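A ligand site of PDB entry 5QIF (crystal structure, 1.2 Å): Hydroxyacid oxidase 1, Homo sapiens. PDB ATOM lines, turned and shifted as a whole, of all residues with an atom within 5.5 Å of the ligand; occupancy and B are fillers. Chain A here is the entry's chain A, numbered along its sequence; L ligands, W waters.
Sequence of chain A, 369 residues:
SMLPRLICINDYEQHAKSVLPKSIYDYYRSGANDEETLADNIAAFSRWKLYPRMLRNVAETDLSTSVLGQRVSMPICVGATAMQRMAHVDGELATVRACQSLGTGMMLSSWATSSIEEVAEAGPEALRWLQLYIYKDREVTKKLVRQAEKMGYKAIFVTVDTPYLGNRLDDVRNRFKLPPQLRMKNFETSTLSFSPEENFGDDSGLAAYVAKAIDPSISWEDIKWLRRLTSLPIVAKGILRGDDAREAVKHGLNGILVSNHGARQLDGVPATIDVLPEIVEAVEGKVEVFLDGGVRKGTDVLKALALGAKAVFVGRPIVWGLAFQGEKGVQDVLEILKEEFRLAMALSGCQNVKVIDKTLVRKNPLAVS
The side-chain hydroxyl (OG) of Ser 259 sits at hydrogen-bond distance from an oxygen (O4) of the ligand (3.3 Å). NZ of Lys 237 sits at hydrogen-bond distance from O1 of the ligand, at 2.9 Å. The guanidinium group (NH1) of Arg 316 is in salt-bridge range of an oxygen (O9) of the ligand (3.0 Å). The guanidinium group of Arg 296 is in salt-bridge range of an oxygen (O8) of the ligand, at 2.8 Å. The backbone NH (N) of Gly 315 is in hydrogen-bond range of an oxygen (O7) of the ligand (2.8 Å). The side-chain amide oxygen (OE1) of Gln 131 lies within hydrogen-bond range of a nitrogen (N2) of the ligand (3.0 Å). A nitrogen (N3) of the ligand lies within hydrogen-bond range of the backbone NH (N) of Ala 82 (3.1 Å). The side-chain carboxylate of Asp 292 is in hydrogen-bond range of an oxygen (O4) of the ligand (2.8 Å). OG of Ser 109 is in hydrogen-bond range of O2 of the ligand, 2.7 Å away. The side-chain hydroxyl of Tyr 133 lies within hydrogen-bond range of a nitrogen (N2) of the ligand (3.3 Å). OG1 of Thr 159 lies within hydrogen-bond range of O1 of the ligand (2.7 Å). O3 of the ligand sits at hydrogen-bond distance from O of Ala 80 (2.6 Å). An oxygen (O9) of the ligand sits at hydrogen-bond distance from the backbone NH of Arg 316. O6 of the ligand sits close to N of Gly 293. The backbone NH of Gly 294 lies within hydrogen-bond range of an oxygen (O8) of the ligand, 2.9 Å away.
O of Ser 30 is in hydrogen-bond range of NH2 of Arg 316. The backbone carbonyl oxygen (O) of Tyr 28 sits at hydrogen-bond distance from the guanidinium group (NH1) of Arg 264, at 3.4 Å. NH1 of Arg 264 is in hydrogen-bond range of O of Ser 30 (2.9 Å). The side-chain hydroxyl (OG) of Ser 259 sits at hydrogen-bond distance from the side-chain carboxylate (OD1) of Asp 292, 2.7 Å away. N of His 261 is in hydrogen-bond range of OG of Ser 259, at 3.0 Å. N of Trp 111 is in hydrogen-bond range of OG of Ser 109 (2.8 Å). O of Val 314 is in hydrogen-bond range of N of Gly 79 (2.9 Å). SD of Met 107 lies within hydrogen-bond range of N of Ala 80 (3.6 Å).
Tyr 27 touches the ligand. CD1 of Tyr 28 touches C7 of the ligand, 3.4 Å away. Thr 81 touches the ligand. Trp 111 touches the ligand. His 261 touches the ligand. Gly 262 touches the ligand. NH2 of Arg 264 touches C6 of the ligand, 3.3 Å away. Val 314 touches the ligand (C to O7, 3.8 Å). Hydrophobic or aromatic side chains that line the ligand: Tyr 27, Tyr 28, Ala 82, Trp 111, Tyr 133 and His 261. Within 4 Å of the ligand: Tyr 27, Tyr 28, Ala 80, Thr 81, Ala 82, Ser 109, Trp 111, Gln 131, Tyr 133, Thr 159, Lys 237, Ser 259, His 261, Gly 262, Arg 264, Asp 292, Gly 293, Gly 294, Arg 296, Val 314, Gly 315 and Arg 316.
Water W3 lies within hydrogen-bond range of an oxygen (O8) of the ligand (2.8 Å), the side-chain amide nitrogen of Asn 41 (2.9 Å), the guanidinium group of Arg 316 (3.1 Å) and the backbone carbonyl oxygen of Gly 262 (3.5 Å). Water W1 lies within hydrogen-bond range of the side-chain carboxylate (OD2) of Asp 292 and an oxygen (O3) of the ligand.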
ATOM      1  N   TYR A  27      21.681  28.427   7.759  1.00  0.00           N
ATOM      2  CA  TYR A  27      21.204  28.325   6.372  1.00  0.00           C
ATOM      3  C   TYR A  27      20.933  26.873   6.011  1.00  0.00           C
ATOM      4  O   TYR A  27      19.902  26.550   5.444  1.00  0.00           O
ATOM      5  CB  TYR A  27      22.231  28.944   5.361  1.00  0.00           C
ATOM      6  CG  TYR A  27      21.930  28.517   3.947  1.00  0.00           C
ATOM      7  CD1 TYR A  27      20.855  29.026   3.253  1.00  0.00           C
ATOM      8  CD2 TYR A  27      22.688  27.514   3.326  1.00  0.00           C
ATOM      9  CE1 TYR A  27      20.506  28.554   2.000  1.00  0.00           C
ATOM     10  CE2 TYR A  27      22.392  27.064   2.058  1.00  0.00           C
ATOM     11  CZ  TYR A  27      21.292  27.574   1.379  1.00  0.00           C
ATOM     12  OH  TYR A  27      20.942  27.073   0.134  1.00  0.00           O
ATOM     13  N   TYR A  28      21.866  25.989   6.362  1.00  0.00           N
ATOM     14  CA  TYR A  28      21.729  24.589   6.019  1.00  0.00           C
ATOM     15  C   TYR A  28      20.637  23.899   6.855  1.00  0.00           C
ATOM     16  O   TYR A  28      19.894  23.061   6.325  1.00  0.00           O
ATOM     17  CB  TYR A  28      23.075  23.887   6.215  1.00  0.00           C
ATOM     18  CG  TYR A  28      24.184  24.200   5.215  1.00  0.00           C
ATOM     19  CD1 TYR A  28      23.957  24.229   3.849  1.00  0.00           C
ATOM     20  CD2 TYR A  28      25.498  24.377   5.667  1.00  0.00           C
ATOM     21  CE1 TYR A  28      25.033  24.453   2.931  1.00  0.00           C
ATOM     22  CE2 TYR A  28      26.564  24.594   4.790  1.00  0.00           C
ATOM     23  CZ  TYR A  28      26.308  24.648   3.441  1.00  0.00           C
ATOM     24  OH  TYR A  28      27.418  24.792   2.621  1.00  0.00           O
ATOM     25  N   SER A  30      17.948  25.199   8.528  1.00  0.00           N
ATOM     26  CA  SER A  30      16.634  25.803   8.675  1.00  0.00           C
ATOM     27  C   SER A  30      15.558  25.184   7.810  1.00  0.00           C
ATOM     28  O   SER A  30      15.808  24.722   6.711  1.00  0.00           O
ATOM     29  CB  SER A  30      16.685  27.285   8.342  1.00  0.00           C
ATOM     30  OG  SER A  30      17.201  28.030   9.438  1.00  0.00           O
ATOM     31  N   ASN A  41       8.941  15.835   8.996  1.00  0.00           N
ATOM     32  CA  ASN A  41       9.636  14.967   8.043  1.00  0.00           C
ATOM     33  C   ASN A  41      10.360  13.837   8.757  1.00  0.00           C
ATOM     34  O   ASN A  41      10.449  12.728   8.218  1.00  0.00           O
ATOM     35  CB  ASN A  41      10.660  15.742   7.171  1.00  0.00           C
ATOM     36  CG  ASN A  41      10.053  16.408   5.963  1.00  0.00           C
ATOM     37  OD1 ASN A  41       8.867  16.207   5.641  1.00  0.00           O
ATOM     38  ND2 ASN A  41      10.847  17.268   5.299  1.00  0.00           N
ATOM     39  N   GLY A  79      20.934  14.317  -2.952  1.00  0.00           N
ATOM     40  CA  GLY A  79      20.058  15.394  -3.449  1.00  0.00           C
ATOM     41  C   GLY A  79      20.775  16.728  -3.587  1.00  0.00           C
ATOM     42  O   GLY A  79      21.820  16.980  -2.959  1.00  0.00           O
ATOM     43  N   ALA A  80      20.177  17.615  -4.384  1.00  0.00           N
ATOM     44  CA  ALA A  80      20.743  18.963  -4.630  1.00  0.00           C
ATOM     45  C   ALA A  80      20.700  19.812  -3.363  1.00  0.00           C
ATOM     46  O   ALA A  80      19.643  19.978  -2.745  1.00  0.00           O
ATOM     47  CB  ALA A  80      19.978  19.667  -5.728  1.00  0.00           C
ATOM     48  N   THR A  81      21.857  20.287  -2.928  1.00  0.00           N
ATOM     49  CA  THR A  81      21.949  21.272  -1.848  1.00  0.00           C
ATOM     50  C   THR A  81      22.894  22.349  -2.332  1.00  0.00           C
ATOM     51  O   THR A  81      24.035  22.079  -2.712  1.00  0.00           O
ATOM     52  CB  THR A  81      22.433  20.673  -0.526  1.00  0.00           C
ATOM     53  OG1 THR A  81      23.611  19.896  -0.739  1.00  0.00           O
ATOM     54  CG2 THR A  81      21.353  19.824   0.161  1.00  0.00           C
ATOM     55  N   ALA A  82      22.401  23.581  -2.367  1.00  0.00           N
ATOM     56  CA  ALA A  82      23.138  24.695  -2.880  1.00  0.00           C
ATOM     57  C   ALA A  82      24.417  25.004  -2.109  1.00  0.00           C
ATOM     58  O   ALA A  82      24.536  24.779  -0.922  1.00  0.00           O
ATOM     59  CB  ALA A  82      22.235  25.917  -2.890  1.00  0.00           C
ATOM     60  N   MET A 107      22.790  14.519  -7.577  1.00  0.00           N
ATOM     61  CA  MET A 107      21.997  15.570  -8.168  1.00  0.00           C
ATOM     62  C   MET A 107      22.676  16.912  -7.878  1.00  0.00           C
ATOM     63  O   MET A 107      22.803  17.297  -6.722  1.00  0.00           O
ATOM     64  CB  MET A 107      20.582  15.537  -7.591  1.00  0.00           C
ATOM     65  CG  MET A 107      19.602  16.482  -8.251  1.00  0.00           C
ATOM     66  SD  MET A 107      18.129  16.834  -7.290  1.00  0.00           S
ATOM     67  CE  MET A 107      17.523  15.178  -6.958  1.00  0.00           C
ATOM     68  N   SER A 109      22.957  20.897  -7.765  1.00  0.00           N
ATOM     69  CA  SER A 109      22.176  22.133  -7.709  1.00  0.00           C
ATOM     70  C   SER A 109      22.478  23.116  -8.824  1.00  0.00           C
ATOM     71  O   SER A 109      23.659  23.365  -9.106  1.00  0.00           O
ATOM     72  CB  SER A 109      22.459  22.828  -6.364  1.00  0.00           C
ATOM     73  OG  SER A 109      21.814  24.094  -6.254  1.00  0.00           O
ATOM     74  N   SER A 110      21.448  23.790  -9.320  1.00  0.00           N
ATOM     75  CA  SER A 110      21.722  24.944 -10.236  1.00  0.00           C
ATOM     76  C   SER A 110      22.469  26.059  -9.507  1.00  0.00           C
ATOM     77  O   SER A 110      23.104  26.918 -10.158  1.00  0.00           O
ATOM     78  CB  SER A 110      20.416  25.512 -10.774  1.00  0.00           C
ATOM     79  OG  SER A 110      19.930  24.749 -11.858  1.00  0.00           O
ATOM     80  N   TRP A 111      22.353  26.107  -8.186  1.00  0.00           N
ATOM     81  CA  TRP A 111      22.992  27.115  -7.293  1.00  0.00           C
ATOM     82  C   TRP A 111      24.277  26.576  -6.636  1.00  0.00           C
ATOM     83  O   TRP A 111      24.665  26.999  -5.567  1.00  0.00           O
ATOM     84  CB  TRP A 111      22.008  27.544  -6.179  1.00  0.00           C
ATOM     85  CG  TRP A 111      20.738  28.170  -6.683  1.00  0.00           C
ATOM     86  CD1 TRP A 111      20.502  28.688  -7.937  1.00  0.00           C
ATOM     87  CD2 TRP A 111      19.519  28.406  -5.938  1.00  0.00           C
ATOM     88  NE1 TRP A 111      19.225  29.201  -8.012  1.00  0.00           N
ATOM     89  CE2 TRP A 111      18.603  29.052  -6.797  1.00  0.00           C
ATOM     90  CE3 TRP A 111      19.106  28.098  -4.630  1.00  0.00           C
ATOM     91  CZ2 TRP A 111      17.315  29.402  -6.376  1.00  0.00           C
ATOM     92  CZ3 TRP A 111      17.855  28.468  -4.220  1.00  0.00           C
ATOM     93  CH2 TRP A 111      16.964  29.083  -5.088  1.00  0.00           C
ATOM     94  N   GLN A 131      19.876  19.402 -11.211  1.00  0.00           N
ATOM     95  CA  GLN A 131      18.653  20.056 -10.698  1.00  0.00           C
ATOM     96  C   GLN A 131      18.586  21.431 -11.368  1.00  0.00           C
ATOM     97  O   GLN A 131      19.565  22.197 -11.351  1.00  0.00           O
ATOM     98  CB  GLN A 131      18.707  20.190  -9.192  1.00  0.00           C
ATOM     99  CG  GLN A 131      17.536  20.950  -8.574  1.00  0.00           C
ATOM    100  CD  GLN A 131      17.775  22.468  -8.587  1.00  0.00           C
ATOM    101  OE1 GLN A 131      18.831  22.944  -8.165  1.00  0.00           O
ATOM    102  NE2 GLN A 131      16.761  23.226  -9.005  1.00  0.00           N
ATOM    103  N   TYR A 133      16.432  25.064 -12.026  1.00  0.00           N
ATOM    104  CA  TYR A 133      15.438  26.111 -11.820  1.00  0.00           C
ATOM    105  C   TYR A 133      15.155  26.797 -13.151  1.00  0.00           C
ATOM    106  O   TYR A 133      16.077  26.982 -13.954  1.00  0.00           O
ATOM    107  CB  TYR A 133      15.967  27.151 -10.802  1.00  0.00           C
ATOM    108  CG  TYR A 133      15.961  26.733  -9.335  1.00  0.00           C
ATOM    109  CD1 TYR A 133      14.746  26.480  -8.716  1.00  0.00           C
ATOM    110  CD2 TYR A 133      17.117  26.564  -8.583  1.00  0.00           C
ATOM    111  CE1 TYR A 133      14.681  26.115  -7.422  1.00  0.00           C
ATOM    112  CE2 TYR A 133      17.055  26.189  -7.247  1.00  0.00           C
ATOM    113  CZ  TYR A 133      15.811  25.982  -6.684  1.00  0.00           C
ATOM    114  OH  TYR A 133      15.630  25.611  -5.376  1.00  0.00           O
ATOM    115  N   THR A 159      12.806  21.684 -10.458  1.00  0.00           N
ATOM    116  CA  THR A 159      12.174  22.052  -9.189  1.00  0.00           C
ATOM    117  C   THR A 159      10.936  22.861  -9.453  1.00  0.00           C
ATOM    118  O   THR A 159      11.012  23.877 -10.170  1.00  0.00           O
ATOM    119  CB  THR A 159      13.173  22.740  -8.276  1.00  0.00           C
ATOM    120  OG1 THR A 159      14.280  21.853  -8.069  1.00  0.00           O
ATOM    121  CG2 THR A 159      12.533  23.108  -6.938  1.00  0.00           C
ATOM    122  N   LYS A 237      10.368  17.675  -9.412  1.00  0.00           N
ATOM    123  CA  LYS A 237      10.834  17.685  -8.009  1.00  0.00           C
ATOM    124  C   LYS A 237      10.015  18.695  -7.213  1.00  0.00           C
ATOM    125  O   LYS A 237       9.995  19.899  -7.516  1.00  0.00           O
ATOM    126  CB  LYS A 237      12.311  18.040  -7.952  1.00  0.00           C
ATOM    127  CG  LYS A 237      12.854  18.228  -6.538  1.00  0.00           C
ATOM    128  CD  LYS A 237      14.342  18.504  -6.546  1.00  0.00           C
ATOM    129  CE  LYS A 237      14.969  18.563  -5.177  1.00  0.00           C
ATOM    130  NZ  LYS A 237      14.672  19.824  -4.517  1.00  0.00           N
ATOM    131  N   SER A 259       8.671  15.606  -2.573  1.00  0.00           N
ATOM    132  CA  SER A 259       9.579  16.490  -1.871  1.00  0.00           C
ATOM    133  C   SER A 259       8.795  17.683  -1.393  1.00  0.00           C
ATOM    134  O   SER A 259       7.963  18.214  -2.118  1.00  0.00           O
ATOM    135  CB  SER A 259      10.724  16.941  -2.789  1.00  0.00           C
ATOM    136  OG  SER A 259      11.599  17.837  -2.129  1.00  0.00           O
ATOM    137  N   HIS A 261      10.906  20.112  -0.309  1.00  0.00           N
ATOM    138  CA  HIS A 261      12.068  20.972  -0.377  1.00  0.00           C
ATOM    139  C   HIS A 261      12.823  21.009   0.966  1.00  0.00           C
ATOM    140  O   HIS A 261      13.271  22.065   1.417  1.00  0.00           O
ATOM    141  CB  HIS A 261      11.693  22.383  -0.896  1.00  0.00           C
ATOM    142  CG  HIS A 261      12.781  23.134  -1.589  1.00  0.00           C
ATOM    143  ND1 HIS A 261      12.653  23.594  -2.886  1.00  0.00           N
ATOM    144  CD2 HIS A 261      13.966  23.615  -1.140  1.00  0.00           C
ATOM    145  CE1 HIS A 261      13.746  24.285  -3.211  1.00  0.00           C
ATOM    146  NE2 HIS A 261      14.551  24.330  -2.172  1.00  0.00           N
ATOM    147  N   GLY A 262      12.887  19.860   1.620  1.00  0.00           N
ATOM    148  CA  GLY A 262      13.495  19.796   2.948  1.00  0.00           C
ATOM    149  C   GLY A 262      12.778  20.696   3.960  1.00  0.00           C
ATOM    150  O   GLY A 262      13.396  21.194   4.914  1.00  0.00           O
ATOM    151  N   ARG A 264      11.577  23.617   3.518  1.00  0.00           N
ATOM    152  CA  ARG A 264      12.101  24.996   3.419  1.00  0.00           C
ATOM    153  C   ARG A 264      11.215  25.952   2.618  1.00  0.00           C
ATOM    154  O   ARG A 264      11.592  27.132   2.471  1.00  0.00           O
ATOM    155  CB  ARG A 264      13.511  24.950   2.782  1.00  0.00           C
ATOM    156  CG  ARG A 264      14.509  24.196   3.657  1.00  0.00           C
ATOM    157  CD  ARG A 264      15.726  23.704   2.921  1.00  0.00           C
ATOM    158  NE  ARG A 264      16.664  24.725   2.476  1.00  0.00           N
ATOM    159  CZ  ARG A 264      17.645  25.224   3.211  1.00  0.00           C
ATOM    160  NH1 ARG A 264      17.732  24.970   4.504  1.00  0.00           N
ATOM    161  NH2 ARG A 264      18.576  25.977   2.620  1.00  0.00           N
ATOM    162  N   ASP A 292      12.439  12.529  -0.961  1.00  0.00           N
ATOM    163  CA  ASP A 292      13.433  13.140  -0.071  1.00  0.00           C
ATOM    164  C   ASP A 292      12.697  13.818   1.061  1.00  0.00           C
ATOM    165  O   ASP A 292      11.471  13.964   1.034  1.00  0.00           O
ATOM    166  CB  ASP A 292      14.419  14.062  -0.823  1.00  0.00           C
ATOM    167  CG  ASP A 292      13.830  15.333  -1.368  1.00  0.00           C
ATOM    168  OD1 ASP A 292      12.841  15.859  -0.844  1.00  0.00           O
ATOM    169  OD2 ASP A 292      14.481  15.888  -2.299  1.00  0.00           O
ATOM    170  N   GLY A 293      13.445  14.217   2.089  1.00  0.00           N
ATOM    171  CA  GLY A 293      12.913  14.889   3.268  1.00  0.00           C
ATOM    172  C   GLY A 293      12.932  14.001   4.506  1.00  0.00           C
ATOM    173  O   GLY A 293      12.062  13.164   4.683  1.00  0.00           O
ATOM    174  N   GLY A 294      13.905  14.246   5.371  1.00  0.00           N
ATOM    175  CA  GLY A 294      13.977  13.561   6.650  1.00  0.00           C
ATOM    176  C   GLY A 294      14.664  12.215   6.665  1.00  0.00           C
ATOM    177  O   GLY A 294      14.632  11.562   7.718  1.00  0.00           O
ATOM    178  N   VAL A 295      15.315  11.814   5.568  1.00  0.00           N
ATOM    179  CA  VAL A 295      16.024  10.527   5.578  1.00  0.00           C
ATOM    180  C   VAL A 295      17.341  10.671   6.340  1.00  0.00           C
ATOM    181  O   VAL A 295      18.217  11.437   5.966  1.00  0.00           O
ATOM    182  CB  VAL A 295      16.256  10.016   4.128  1.00  0.00           C
ATOM    183  CG1 VAL A 295      17.118   8.770   4.157  1.00  0.00           C
ATOM    184  CG2 VAL A 295      14.959   9.796   3.365  1.00  0.00           C
ATOM    185  N   ARG A 296      17.437   9.912   7.439  1.00  0.00           N
ATOM    186  CA  ARG A 296      18.596   9.957   8.329  1.00  0.00           C
ATOM    187  C   ARG A 296      19.126   8.589   8.674  1.00  0.00           C
ATOM    188  O   ARG A 296      20.262   8.489   9.168  1.00  0.00           O
ATOM    189  CB  ARG A 296      18.252  10.685   9.620  1.00  0.00           C
ATOM    190  CG  ARG A 296      17.669  12.088   9.469  1.00  0.00           C
ATOM    191  CD  ARG A 296      18.652  13.100   8.950  1.00  0.00           C
ATOM    192  NE  ARG A 296      18.013  14.415   8.763  1.00  0.00           N
ATOM    193  CZ  ARG A 296      17.586  14.920   7.613  1.00  0.00           C
ATOM    194  NH1 ARG A 296      17.703  14.255   6.469  1.00  0.00           N
ATOM    195  NH2 ARG A 296      17.090  16.147   7.586  1.00  0.00           N
ATOM    196  N   PHE A 313      16.600  10.386  -1.806  1.00  0.00           N
ATOM    197  CA  PHE A 313      17.669  11.365  -1.863  1.00  0.00           C
ATOM    198  C   PHE A 313      17.869  11.969  -0.479  1.00  0.00           C
ATOM    199  O   PHE A 313      16.900  12.151   0.290  1.00  0.00           O
ATOM    200  CB  PHE A 313      17.341  12.465  -2.873  1.00  0.00           C
ATOM    201  CG  PHE A 313      17.281  11.973  -4.298  1.00  0.00           C
ATOM    202  CD1 PHE A 313      18.372  12.109  -5.141  1.00  0.00           C
ATOM    203  CD2 PHE A 313      16.166  11.336  -4.788  1.00  0.00           C
ATOM    204  CE1 PHE A 313      18.363  11.611  -6.442  1.00  0.00           C
ATOM    205  CE2 PHE A 313      16.141  10.848  -6.076  1.00  0.00           C
ATOM    206  CZ  PHE A 313      17.233  10.995  -6.911  1.00  0.00           C
ATOM    207  N   VAL A 314      19.146  12.243  -0.154  1.00  0.00           N
ATOM    208  CA  VAL A 314      19.532  12.866   1.091  1.00  0.00           C
ATOM    209  C   VAL A 314      20.116  14.226   0.810  1.00  0.00           C
ATOM    210  O   VAL A 314      20.963  14.377  -0.090  1.00  0.00           O
ATOM    211  CB  VAL A 314      20.477  12.005   1.957  1.00  0.00           C
ATOM    212  CG1 VAL A 314      19.681  10.904   2.675  1.00  0.00           C
ATOM    213  CG2 VAL A 314      21.607  11.509   1.174  1.00  0.00           C
ATOM    214  N   GLY A 315      19.673  15.202   1.590  1.00  0.00           N
ATOM    215  CA  GLY A 315      20.132  16.572   1.475  1.00  0.00           C
ATOM    216  C   GLY A 315      21.108  16.916   2.556  1.00  0.00           C
ATOM    217  O   GLY A 315      22.321  16.794   2.372  1.00  0.00           O
ATOM    218  N   ARG A 316      20.616  17.352   3.708  1.00  0.00           N
ATOM    219  CA  ARG A 316      21.469  17.863   4.781  1.00  0.00           C
ATOM    220  C   ARG A 316      22.585  16.903   5.228  1.00  0.00           C
ATOM    221  O   ARG A 316      23.689  17.379   5.509  1.00  0.00           O
ATOM    222  CB  ARG A 316      20.618  18.300   5.972  1.00  0.00           C
ATOM    223  CG  ARG A 316      19.762  19.526   5.702  1.00  0.00           C
ATOM    224  CD  ARG A 316      18.910  19.866   6.861  1.00  0.00           C
ATOM    225  NE  ARG A 316      17.966  20.958   6.579  1.00  0.00           N
ATOM    226  CZ  ARG A 316      16.713  20.808   6.116  1.00  0.00           C
ATOM    227  NH1 ARG A 316      16.253  19.617   5.739  1.00  0.00           N
ATOM    228  NH2 ARG A 316      15.942  21.876   6.052  1.00  0.00           N
ATOM    229  N   PRO A 317      22.324  15.585   5.312  1.00  0.00           N
ATOM    230  CA  PRO A 317      23.427  14.708   5.803  1.00  0.00           C
ATOM    231  C   PRO A 317      24.715  14.862   4.994  1.00  0.00           C
ATOM    232  O   PRO A 317      25.819  14.720   5.548  1.00  0.00           O
ATOM    233  CB  PRO A 317      22.828  13.314   5.694  1.00  0.00           C
ATOM    234  CG  PRO A 317      21.371  13.600   6.041  1.00  0.00           C
ATOM    235  CD  PRO A 317      21.056  14.846   5.254  1.00  0.00           C
ATOM    236  N   VAL A 319      25.840  17.592   3.475  1.00  0.00           N
ATOM    237  CA  VAL A 319      26.496  18.839   3.895  1.00  0.00           C
ATOM    238  C   VAL A 319      27.231  18.642   5.216  1.00  0.00           C
ATOM    239  O   VAL A 319      28.341  19.159   5.415  1.00  0.00           O
ATOM    240  CB  VAL A 319      25.451  19.974   3.964  1.00  0.00           C
ATOM    241  CG1 VAL A 319      26.056  21.235   4.519  1.00  0.00           C
ATOM    242  CG2 VAL A 319      24.777  20.161   2.624  1.00  0.00           C
HETATM  243  N1  LIG L   1      16.554  21.923  -3.769  1.00  0.00           N
HETATM  244  C1  LIG L   1      16.764  22.361  -5.040  1.00  0.00           C
HETATM  245  O1  LIG L   1      15.952  21.981  -5.899  1.00  0.00           O
HETATM  246  N2  LIG L   1      17.837  23.147  -5.341  1.00  0.00           N
HETATM  247  C2  LIG L   1      18.687  23.627  -4.446  1.00  0.00           C
HETATM  248  O2  LIG L   1      19.618  24.345  -4.779  1.00  0.00           O
HETATM  249  C3  LIG L   1      18.531  23.224  -3.051  1.00  0.00           C
HETATM  250  N3  LIG L   1      19.360  23.670  -2.099  1.00  0.00           N
HETATM  251  C4  LIG L   1      19.222  23.226  -0.829  1.00  0.00           C
HETATM  252  C5  LIG L   1      20.105  23.661   0.173  1.00  0.00           C
HETATM  253  C6  LIG L   1      19.953  23.175   1.461  1.00  0.00           C
HETATM  254  C7  LIG L   1      20.922  23.615   2.510  1.00  0.00           C
HETATM  255  C8  LIG L   1      18.862  22.246   1.794  1.00  0.00           C
HETATM  256  C9  LIG L   1      18.748  21.738   3.217  1.00  0.00           C
HETATM  257  C10 LIG L   1      17.994  21.819   0.802  1.00  0.00           C
HETATM  258  C11 LIG L   1      18.118  22.300  -0.499  1.00  0.00           C
HETATM  259  N4  LIG L   1      17.226  21.885  -1.505  1.00  0.00           N
HETATM  260  C12 LIG L   1      17.409  22.334  -2.804  1.00  0.00           C
HETATM  261  C13 LIG L   1      16.204  20.870  -1.233  1.00  0.00           C
HETATM  262  C14 LIG L   1      16.905  19.468  -1.305  1.00  0.00           C
HETATM  263  O3  LIG L   1      17.147  19.094  -2.696  1.00  0.00           O
HETATM  264  C15 LIG L   1      16.102  18.327  -0.698  1.00  0.00           C
HETATM  265  O4  LIG L   1      14.757  18.405  -1.207  1.00  0.00           O
HETATM  266  C16 LIG L   1      16.092  18.336   0.833  1.00  0.00           C
HETATM  267  O5  LIG L   1      17.397  18.694   1.315  1.00  0.00           O
HETATM  268  C17 LIG L   1      15.750  16.963   1.341  1.00  0.00           C
HETATM  269  O6  LIG L   1      15.558  16.910   2.757  1.00  0.00           O
HETATM  270  P1  LIG L   1      16.742  16.547   3.807  1.00  0.00           P
HETATM  271  O7  LIG L   1      17.477  15.315   3.373  1.00  0.00           O
HETATM  272  O8  LIG L   1      15.921  16.335   5.045  1.00  0.00           O
HETATM  273  O9  LIG L   1      17.669  17.730   3.925  1.00  0.00           O
HETATM  274  O   HOH W   1      16.999  16.280  -3.488  1.00  0.00           O
HETATM  275  O   HOH W   2      15.974  13.165   2.772  1.00  0.00           O
HETATM  276  O   HOH W   3      13.691  17.851   5.822  1.00  0.00           O
